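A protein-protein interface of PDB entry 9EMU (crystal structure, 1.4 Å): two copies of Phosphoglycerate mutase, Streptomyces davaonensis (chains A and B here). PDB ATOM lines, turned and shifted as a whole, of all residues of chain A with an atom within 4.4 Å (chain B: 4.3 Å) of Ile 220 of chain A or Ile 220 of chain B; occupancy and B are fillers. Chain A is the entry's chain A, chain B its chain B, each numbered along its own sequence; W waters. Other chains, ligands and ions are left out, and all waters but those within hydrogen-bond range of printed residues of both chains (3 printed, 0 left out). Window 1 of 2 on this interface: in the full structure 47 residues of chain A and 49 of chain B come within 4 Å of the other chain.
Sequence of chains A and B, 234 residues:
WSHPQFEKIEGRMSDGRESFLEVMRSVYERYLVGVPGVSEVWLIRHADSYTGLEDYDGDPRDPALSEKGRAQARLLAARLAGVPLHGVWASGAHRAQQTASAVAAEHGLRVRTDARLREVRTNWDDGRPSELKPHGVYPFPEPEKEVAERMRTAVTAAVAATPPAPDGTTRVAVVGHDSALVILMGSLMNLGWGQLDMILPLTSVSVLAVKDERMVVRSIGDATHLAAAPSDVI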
ATOM      1  N   MET A 185     -25.781  -7.265 -14.198  1.00  0.00           N
ATOM      2  CA  MET A 185     -24.530  -6.524 -14.104  1.00  0.00           C
ATOM      3  C   MET A 185     -24.435  -5.753 -12.795  1.00  0.00           C
ATOM      4  O   MET A 185     -23.371  -5.723 -12.159  1.00  0.00           O
ATOM      5  CB  MET A 185     -24.339  -5.646 -15.332  1.00  0.00           C
ATOM      6  CG  MET A 185     -24.013  -6.494 -16.548  1.00  0.00           C
ATOM      7  SD  MET A 185     -23.627  -5.529 -18.000  1.00  0.00           S
ATOM      8  CE  MET A 185     -25.272  -5.189 -18.585  1.00  0.00           C
ATOM      9  N   MET A 189     -21.672  -6.281  -9.377  1.00  0.00           N
ATOM     10  CA  MET A 189     -20.966  -5.200  -8.706  1.00  0.00           C
ATOM     11  C   MET A 189     -21.526  -4.914  -7.318  1.00  0.00           C
ATOM     12  O   MET A 189     -21.208  -3.872  -6.733  1.00  0.00           O
ATOM     13  CB  MET A 189     -20.991  -3.943  -9.570  1.00  0.00           C
ATOM     14  CG  MET A 189     -20.031  -4.004 -10.742  1.00  0.00           C
ATOM     15  SD  MET A 189     -20.007  -2.454 -11.650  1.00  0.00           S
ATOM     16  CE  MET A 189     -21.354  -2.721 -12.785  1.00  0.00           C
ATOM     17  N   LEU A 196     -26.648   1.280 -10.695  1.00  0.00           N
ATOM     18  CA  LEU A 196     -26.197   1.262 -12.083  1.00  0.00           C
ATOM     19  C   LEU A 196     -27.366   1.750 -12.918  1.00  0.00           C
ATOM     20  O   LEU A 196     -28.218   0.970 -13.353  1.00  0.00           O
ATOM     21  CB  LEU A 196     -25.805  -0.154 -12.488  1.00  0.00           C
ATOM     22  CG  LEU A 196     -25.145  -0.296 -13.850  1.00  0.00           C
ATOM     23  CD1 LEU A 196     -23.805   0.447 -13.862  1.00  0.00           C
ATOM     24  CD2 LEU A 196     -24.977  -1.786 -14.161  1.00  0.00           C
ATOM     25  N   MET A 198     -28.862   2.831 -15.854  1.00  0.00           N
ATOM     26  CA  MET A 198     -28.657   2.774 -17.291  1.00  0.00           C
ATOM     27  C   MET A 198     -29.767   1.961 -17.931  1.00  0.00           C
ATOM     28  O   MET A 198     -30.255   0.985 -17.357  1.00  0.00           O
ATOM     29  CB  MET A 198     -27.309   2.112 -17.635  1.00  0.00           C
ATOM     30  CG  MET A 198     -26.113   2.854 -17.094  1.00  0.00           C
ATOM     31  SD  MET A 198     -24.555   2.009 -17.406  1.00  0.00           S
ATOM     32  CE  MET A 198     -24.458   2.171 -19.185  1.00  0.00           C
ATOM     33  N   LEU A 200     -30.057  -0.268 -21.340  1.00  0.00           N
ATOM     34  CA  LEU A 200     -29.194  -0.844 -22.362  1.00  0.00           C
ATOM     35  C   LEU A 200     -29.833  -0.642 -23.729  1.00  0.00           C
ATOM     36  O   LEU A 200     -30.989  -1.027 -23.925  1.00  0.00           O
ATOM     37  CB  LEU A 200     -28.984  -2.336 -22.109  1.00  0.00           C
ATOM     38  CG  LEU A 200     -28.323  -2.660 -20.766  1.00  0.00           C
ATOM     39  CD1 LEU A 200     -28.232  -4.171 -20.588  1.00  0.00           C
ATOM     40  CD2 LEU A 200     -26.938  -2.006 -20.609  1.00  0.00           C
ATOM     41  N   VAL A 205     -23.960  -4.254 -26.767  1.00  0.00           N
ATOM     42  CA  VAL A 205     -23.032  -5.281 -26.318  1.00  0.00           C
ATOM     43  C   VAL A 205     -22.477  -4.852 -24.974  1.00  0.00           C
ATOM     44  O   VAL A 205     -21.965  -3.726 -24.834  1.00  0.00           O
ATOM     45  CB  VAL A 205     -21.886  -5.452 -27.330  1.00  0.00           C
ATOM     46  CG1 VAL A 205     -20.821  -6.405 -26.783  1.00  0.00           C
ATOM     47  CG2 VAL A 205     -22.442  -5.906 -28.670  1.00  0.00           C
ATOM     48  N   SER A 206     -22.574  -5.744 -23.996  1.00  0.00           N
ATOM     49  CA  SER A 206     -21.919  -5.602 -22.704  1.00  0.00           C
ATOM     50  C   SER A 206     -21.045  -6.829 -22.503  1.00  0.00           C
ATOM     51  O   SER A 206     -21.418  -7.931 -22.908  1.00  0.00           O
ATOM     52  CB  SER A 206     -22.942  -5.512 -21.584  1.00  0.00           C
ATOM     53  OG  SER A 206     -23.888  -4.470 -21.814  1.00  0.00           O
ATOM     54  N   VAL A 217     -17.573  -7.288 -14.566  1.00  0.00           N
ATOM     55  CA  VAL A 217     -18.190  -6.452 -15.592  1.00  0.00           C
ATOM     56  C   VAL A 217     -17.099  -5.641 -16.295  1.00  0.00           C
ATOM     57  O   VAL A 217     -16.497  -4.734 -15.711  1.00  0.00           O
ATOM     58  CB  VAL A 217     -19.281  -5.541 -15.026  1.00  0.00           C
ATOM     59  CG1 VAL A 217     -19.933  -4.760 -16.189  1.00  0.00           C
ATOM     60  CG2 VAL A 217     -20.318  -6.381 -14.317  1.00  0.00           C
ATOM     61  N   SER A 219     -17.517  -4.151 -19.694  1.00  0.00           N
ATOM     62  CA  SER A 219     -18.047  -3.022 -20.452  1.00  0.00           C
ATOM     63  C   SER A 219     -19.556  -3.174 -20.507  1.00  0.00           C
ATOM     64  O   SER A 219     -20.090  -4.283 -20.351  1.00  0.00           O
ATOM     65  CB  SER A 219     -17.457  -2.946 -21.867  1.00  0.00           C
ATOM     66  OG  SER A 219     -17.737  -4.114 -22.607  1.00  0.00           O
ATOM     67  N   ILE A 220     -20.248  -2.044 -20.708  1.00  0.00           N
ATOM     68  CA  ILE A 220     -21.704  -2.001 -20.563  1.00  0.00           C
ATOM     69  C   ILE A 220     -22.330  -1.153 -21.658  1.00  0.00           C
ATOM     70  O   ILE A 220     -21.971   0.018 -21.819  1.00  0.00           O
ATOM     71  CB  ILE A 220     -22.126  -1.399 -19.208  1.00  0.00           C
ATOM     72  CG1 ILE A 220     -21.448  -2.109 -18.042  1.00  0.00           C
ATOM     73  CG2 ILE A 220     -23.656  -1.467 -19.048  1.00  0.00           C
ATOM     74  CD1 ILE A 220     -21.666  -1.425 -16.729  1.00  0.00           C
ATOM     75  N   GLY A 221     -23.309  -1.721 -22.365  1.00  0.00           N
ATOM     76  CA  GLY A 221     -24.290  -0.939 -23.102  1.00  0.00           C
ATOM     77  C   GLY A 221     -23.867  -0.358 -24.434  1.00  0.00           C
ATOM     78  O   GLY A 221     -24.491   0.607 -24.904  1.00  0.00           O
ATOM     79  N   ASP A 222     -22.827  -0.895 -25.071  1.00  0.00           N
ATOM     80  CA  ASP A 222     -22.275  -0.258 -26.262  1.00  0.00           C
ATOM     81  C   ASP A 222     -23.095  -0.609 -27.501  1.00  0.00           C
ATOM     82  O   ASP A 222     -23.153  -1.777 -27.912  1.00  0.00           O
ATOM     83  CB  ASP A 222     -20.810  -0.648 -26.431  1.00  0.00           C
ATOM     84  CG  ASP A 222     -20.178  -0.011 -27.657  1.00  0.00           C
ATOM     85  OD1 ASP A 222     -20.682  -0.217 -28.771  1.00  0.00           O
ATOM     86  OD2 ASP A 222     -19.164   0.707 -27.505  1.00  0.00           O
ATOM     87  N   MET B 185     -17.912   9.235 -14.781  1.00  0.00           N
ATOM     88  CA  MET B 185     -19.102   8.445 -15.055  1.00  0.00           C
ATOM     89  C   MET B 185     -19.792   8.001 -13.771  1.00  0.00           C
ATOM     90  O   MET B 185     -21.031   8.029 -13.687  1.00  0.00           O
ATOM     91  CB  MET B 185     -18.766   7.282 -15.976  1.00  0.00           C
ATOM     92  CG  MET B 185     -18.499   7.760 -17.395  1.00  0.00           C
ATOM     93  SD  MET B 185     -18.204   6.430 -18.567  1.00  0.00           S
ATOM     94  CE  MET B 185     -16.518   5.996 -18.155  1.00  0.00           C
ATOM     95  N   MET B 189     -23.796   9.273 -12.121  1.00  0.00           N
ATOM     96  CA  MET B 189     -24.787   8.362 -11.565  1.00  0.00           C
ATOM     97  C   MET B 189     -24.891   8.485 -10.050  1.00  0.00           C
ATOM     98  O   MET B 189     -25.508   7.628  -9.400  1.00  0.00           O
ATOM     99  CB  MET B 189     -24.456   6.928 -11.983  1.00  0.00           C
ATOM    100  CG  MET B 189     -24.528   6.755 -13.475  1.00  0.00           C
ATOM    101  SD  MET B 189     -24.474   5.013 -13.918  1.00  0.00           S
ATOM    102  CE  MET B 189     -22.735   4.831 -14.247  1.00  0.00           C
ATOM    103  N   LEU B 196     -19.050   2.044  -9.014  1.00  0.00           N
ATOM    104  CA  LEU B 196     -18.839   1.701 -10.421  1.00  0.00           C
ATOM    105  C   LEU B 196     -17.450   1.086 -10.490  1.00  0.00           C
ATOM    106  O   LEU B 196     -16.450   1.772 -10.708  1.00  0.00           O
ATOM    107  CB  LEU B 196     -18.964   2.939 -11.300  1.00  0.00           C
ATOM    108  CG  LEU B 196     -18.921   2.664 -12.804  1.00  0.00           C
ATOM    109  CD1 LEU B 196     -20.106   1.800 -13.202  1.00  0.00           C
ATOM    110  CD2 LEU B 196     -18.905   3.962 -13.595  1.00  0.00           C
ATOM    111  N   MET B 198     -14.842  -0.622 -11.959  1.00  0.00           N
ATOM    112  CA  MET B 198     -14.386  -0.961 -13.299  1.00  0.00           C
ATOM    113  C   MET B 198     -13.076  -0.255 -13.607  1.00  0.00           C
ATOM    114  O   MET B 198     -12.841   0.877 -13.180  1.00  0.00           O
ATOM    115  CB  MET B 198     -15.415  -0.500 -14.350  1.00  0.00           C
ATOM    116  CG  MET B 198     -16.753  -1.204 -14.287  1.00  0.00           C
ATOM    117  SD  MET B 198     -17.935  -0.499 -15.453  1.00  0.00           S
ATOM    118  CE  MET B 198     -17.371  -1.260 -16.974  1.00  0.00           C
ATOM    119  N   LEU B 200     -11.177   0.995 -17.066  1.00  0.00           N
ATOM    120  CA  LEU B 200     -11.466   1.171 -18.484  1.00  0.00           C
ATOM    121  C   LEU B 200     -10.269   0.704 -19.301  1.00  0.00           C
ATOM    122  O   LEU B 200      -9.151   1.170 -19.065  1.00  0.00           O
ATOM    123  CB  LEU B 200     -11.727   2.627 -18.802  1.00  0.00           C
ATOM    124  CG  LEU B 200     -12.862   3.294 -18.053  1.00  0.00           C
ATOM    125  CD1 LEU B 200     -12.963   4.752 -18.447  1.00  0.00           C
ATOM    126  CD2 LEU B 200     -14.148   2.581 -18.375  1.00  0.00           C
ATOM    127  N   VAL B 205     -14.030   2.866 -25.443  1.00  0.00           N
ATOM    128  CA  VAL B 205     -15.006   3.903 -25.768  1.00  0.00           C
ATOM    129  C   VAL B 205     -16.148   3.820 -24.767  1.00  0.00           C
ATOM    130  O   VAL B 205     -16.711   2.739 -24.546  1.00  0.00           O
ATOM    131  CB  VAL B 205     -15.538   3.714 -27.199  1.00  0.00           C
ATOM    132  CG1 VAL B 205     -16.611   4.759 -27.517  1.00  0.00           C
ATOM    133  CG2 VAL B 205     -14.388   3.803 -28.193  1.00  0.00           C
ATOM    134  N   SER B 206     -16.514   4.970 -24.205  1.00  0.00           N
ATOM    135  CA  SER B 206     -17.661   5.152 -23.322  1.00  0.00           C
ATOM    136  C   SER B 206     -18.455   6.328 -23.877  1.00  0.00           C
ATOM    137  O   SER B 206     -17.868   7.307 -24.334  1.00  0.00           O
ATOM    138  CB  SER B 206     -17.194   5.503 -21.916  1.00  0.00           C
ATOM    139  OG  SER B 206     -16.316   4.500 -21.425  1.00  0.00           O
ATOM    140  N   VAL B 217     -24.910   8.795 -18.694  1.00  0.00           N
ATOM    141  CA  VAL B 217     -23.993   7.730 -19.096  1.00  0.00           C
ATOM    142  C   VAL B 217     -24.758   6.711 -19.931  1.00  0.00           C
ATOM    143  O   VAL B 217     -25.692   6.063 -19.435  1.00  0.00           O
ATOM    144  CB  VAL B 217     -23.356   7.043 -17.878  1.00  0.00           C
ATOM    145  CG1 VAL B 217     -22.391   5.941 -18.352  1.00  0.00           C
ATOM    146  CG2 VAL B 217     -22.614   8.061 -16.997  1.00  0.00           C
ATOM    147  N   SER B 219     -22.952   4.302 -22.209  1.00  0.00           N
ATOM    148  CA  SER B 219     -22.198   3.059 -22.307  1.00  0.00           C
ATOM    149  C   SER B 219     -20.830   3.291 -21.700  1.00  0.00           C
ATOM    150  O   SER B 219     -20.365   4.426 -21.596  1.00  0.00           O
ATOM    151  CB  SER B 219     -22.091   2.560 -23.750  1.00  0.00           C
ATOM    152  OG  SER B 219     -21.400   3.496 -24.546  1.00  0.00           O
ATOM    153  N   ILE B 220     -20.188   2.203 -21.285  1.00  0.00           N
ATOM    154  CA  ILE B 220     -18.952   2.311 -20.511  1.00  0.00           C
ATOM    155  C   ILE B 220     -17.957   1.243 -20.945  1.00  0.00           C
ATOM    156  O   ILE B 220     -18.273   0.052 -20.916  1.00  0.00           O
ATOM    157  CB  ILE B 220     -19.221   2.112 -19.011  1.00  0.00           C
ATOM    158  CG1 ILE B 220     -20.347   3.021 -18.511  1.00  0.00           C
ATOM    159  CG2 ILE B 220     -17.928   2.268 -18.228  1.00  0.00           C
ATOM    160  CD1 ILE B 220     -20.701   2.751 -17.062  1.00  0.00           C
ATOM    161  N   GLY B 221     -16.737   1.667 -21.304  1.00  0.00           N
ATOM    162  CA  GLY B 221     -15.573   0.783 -21.281  1.00  0.00           C
ATOM    163  C   GLY B 221     -15.400  -0.206 -22.416  1.00  0.00           C
ATOM    164  O   GLY B 221     -14.682  -1.198 -22.243  1.00  0.00           O
ATOM    165  N   ASP B 222     -15.979   0.050 -23.584  1.00  0.00           N
ATOM    166  CA  ASP B 222     -15.978  -0.928 -24.670  1.00  0.00           C
ATOM    167  C   ASP B 222     -14.660  -0.876 -25.446  1.00  0.00           C
ATOM    168  O   ASP B 222     -14.363   0.120 -26.101  1.00  0.00           O
ATOM    169  CB  ASP B 222     -17.163  -0.655 -25.600  1.00  0.00           C
ATOM    170  CG  ASP B 222     -17.256  -1.655 -26.742  1.00  0.00           C
ATOM    171  OD1 ASP B 222     -16.314  -1.746 -27.557  1.00  0.00           O
ATOM    172  OD2 ASP B 222     -18.273  -2.348 -26.831  1.00  0.00           O
HETATM  173  O   HOH W   1     -23.224   3.147 -26.921  1.00  0.00           O
HETATM  174  O   HOH W   2     -19.272   2.324 -25.388  1.00  0.00           O
HETATM  175  O   HOH W   3     -19.290  -3.324 -24.568  1.00  0.00           O
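The backbone carbonyl oxygen (O) of Ile 220 of chain A lies within hydrogen-bond range of the backbone NH (N) of Ile 220 of chain B, 2.9 Å away. OD2 of Asp 222 of chain B lies close to OD2 of Asp 222 of chain A.
Leu 196 of chain A touches its own counterpart, Leu 196 of chain B. Met 198 of chain A touches Ser 219 of chain B, and with the chains exchanged Ser 219 of chain A touches Met 198 of chain B. Ile 220 of chain B touches its own counterpart, Ile 220 of chain A. Asp 222 of chain A touches its own counterpart, Asp 222 of chain B. 12 positions are printed for both chains. Of the 14 pairs that touch across the chains among the printed residues, 13 have their exchanged pair printed and touching as well.
Among the printed residues, merely in contact across the chains: Leu 196 of chain A with Leu 196 of chain B (3.99 Å), Met 198 of chain A with Val 217 of chain B (3.99 Å), Met 198 of chain A with Ser 219 of chain B (3.96 Å), Met 198 of chain A with Ile 220 of chain B (3.9 Å), Val 217 of chain A with Met 198 of chain B (3.8 Å), Ser 219 of chain A with Met 198 of chain B (3.96 Å), Ser 219 of chain A with Ile 220 of chain B (3.1 Å), Ser 219 of chain A with Gly 221 of chain B (3.3 Å), Ser 219 of chain A with Asp 222 of chain B (3.8 Å), Ile 220 of chain A with Ser 219 of chain B (3.1 Å), Gly 221 of chain A with Ser 219 of chain B (3.3 Å) and Asp 222 of chain A with Ser 219 of chain B (3.8 Å).
Of the 12 printed residues of chain A, 7 touch a printed residue of chain B. Of the 12 printed residues of chain B, 7 touch a printed residue of chain A. Along chain B the printed residues that touch a printed residue of chain A span positions 196 to 222. Among the printed residues, no Asp or Glu carboxylate lies within 4 Å of a Lys or Arg side-chain nitrogen of the other chain.
Water W2 lies within hydrogen-bond range of OG of Ser 219 of chain B (2.6 Å), OD2 of Asp 222 of chain A (2.7 Å) and O of Val 205 of chain B (2.7 Å). Water W3 lies within hydrogen-bond range of OG of Ser 219 of chain A (2.6 Å), OD2 of Asp 222 of chain B (2.7 Å) and O of Val 205 of chain A (2.7 Å). Water W1 bridges OG of Ser 219 of chain B and O of Gly 221 of chain A.
N of Gly 221 of chain A sits at hydrogen-bond distance from O of Val 205 of chain A (3.5 Å). The backbone NH (N) of Val 205 of chain A is in hydrogen-bond range of the backbone carbonyl oxygen (O) of Asp 222 of chain A, at 2.8 Å. OG of Ser 206 of chain A lies within hydrogen-bond range of N of Gly 221 of chain A (2.9 Å). The backbone carbonyl oxygen of Val 205 of chain B sits at hydrogen-bond distance from the backbone NH of Gly 221 of chain B, at 3.4 Å. N of Val 205 of chain B lies within hydrogen-bond range of O of Asp 222 of chain B (2.8 Å). The side-chain hydroxyl (OG) of Ser 206 of chain B is in hydrogen-bond range of the backbone NH (N) of Gly 221 of chain B.
Ile 220 of chain A touches two residues of chain B. Of the printed residues of chain A, Ile 220 of chain B touches Met 198 (3.9 Å), Ser 219 (3.1 Å) and Ile 220 (2.9 Å). Of the printed residues of chain B, Leu 196 of chain A touches Leu 196 (3.99 Å). Printed residues of chain A within 4 Å of Leu 196 of chain B: Leu 196. The nearest residue of chain B that does not touch Ile 220 of chain A is Met 198 of chain B (4.1 Å). The nearest printed residue of chain A that does not touch Ile 220 of chain B is Leu 196 of chain A (5.0 Å).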
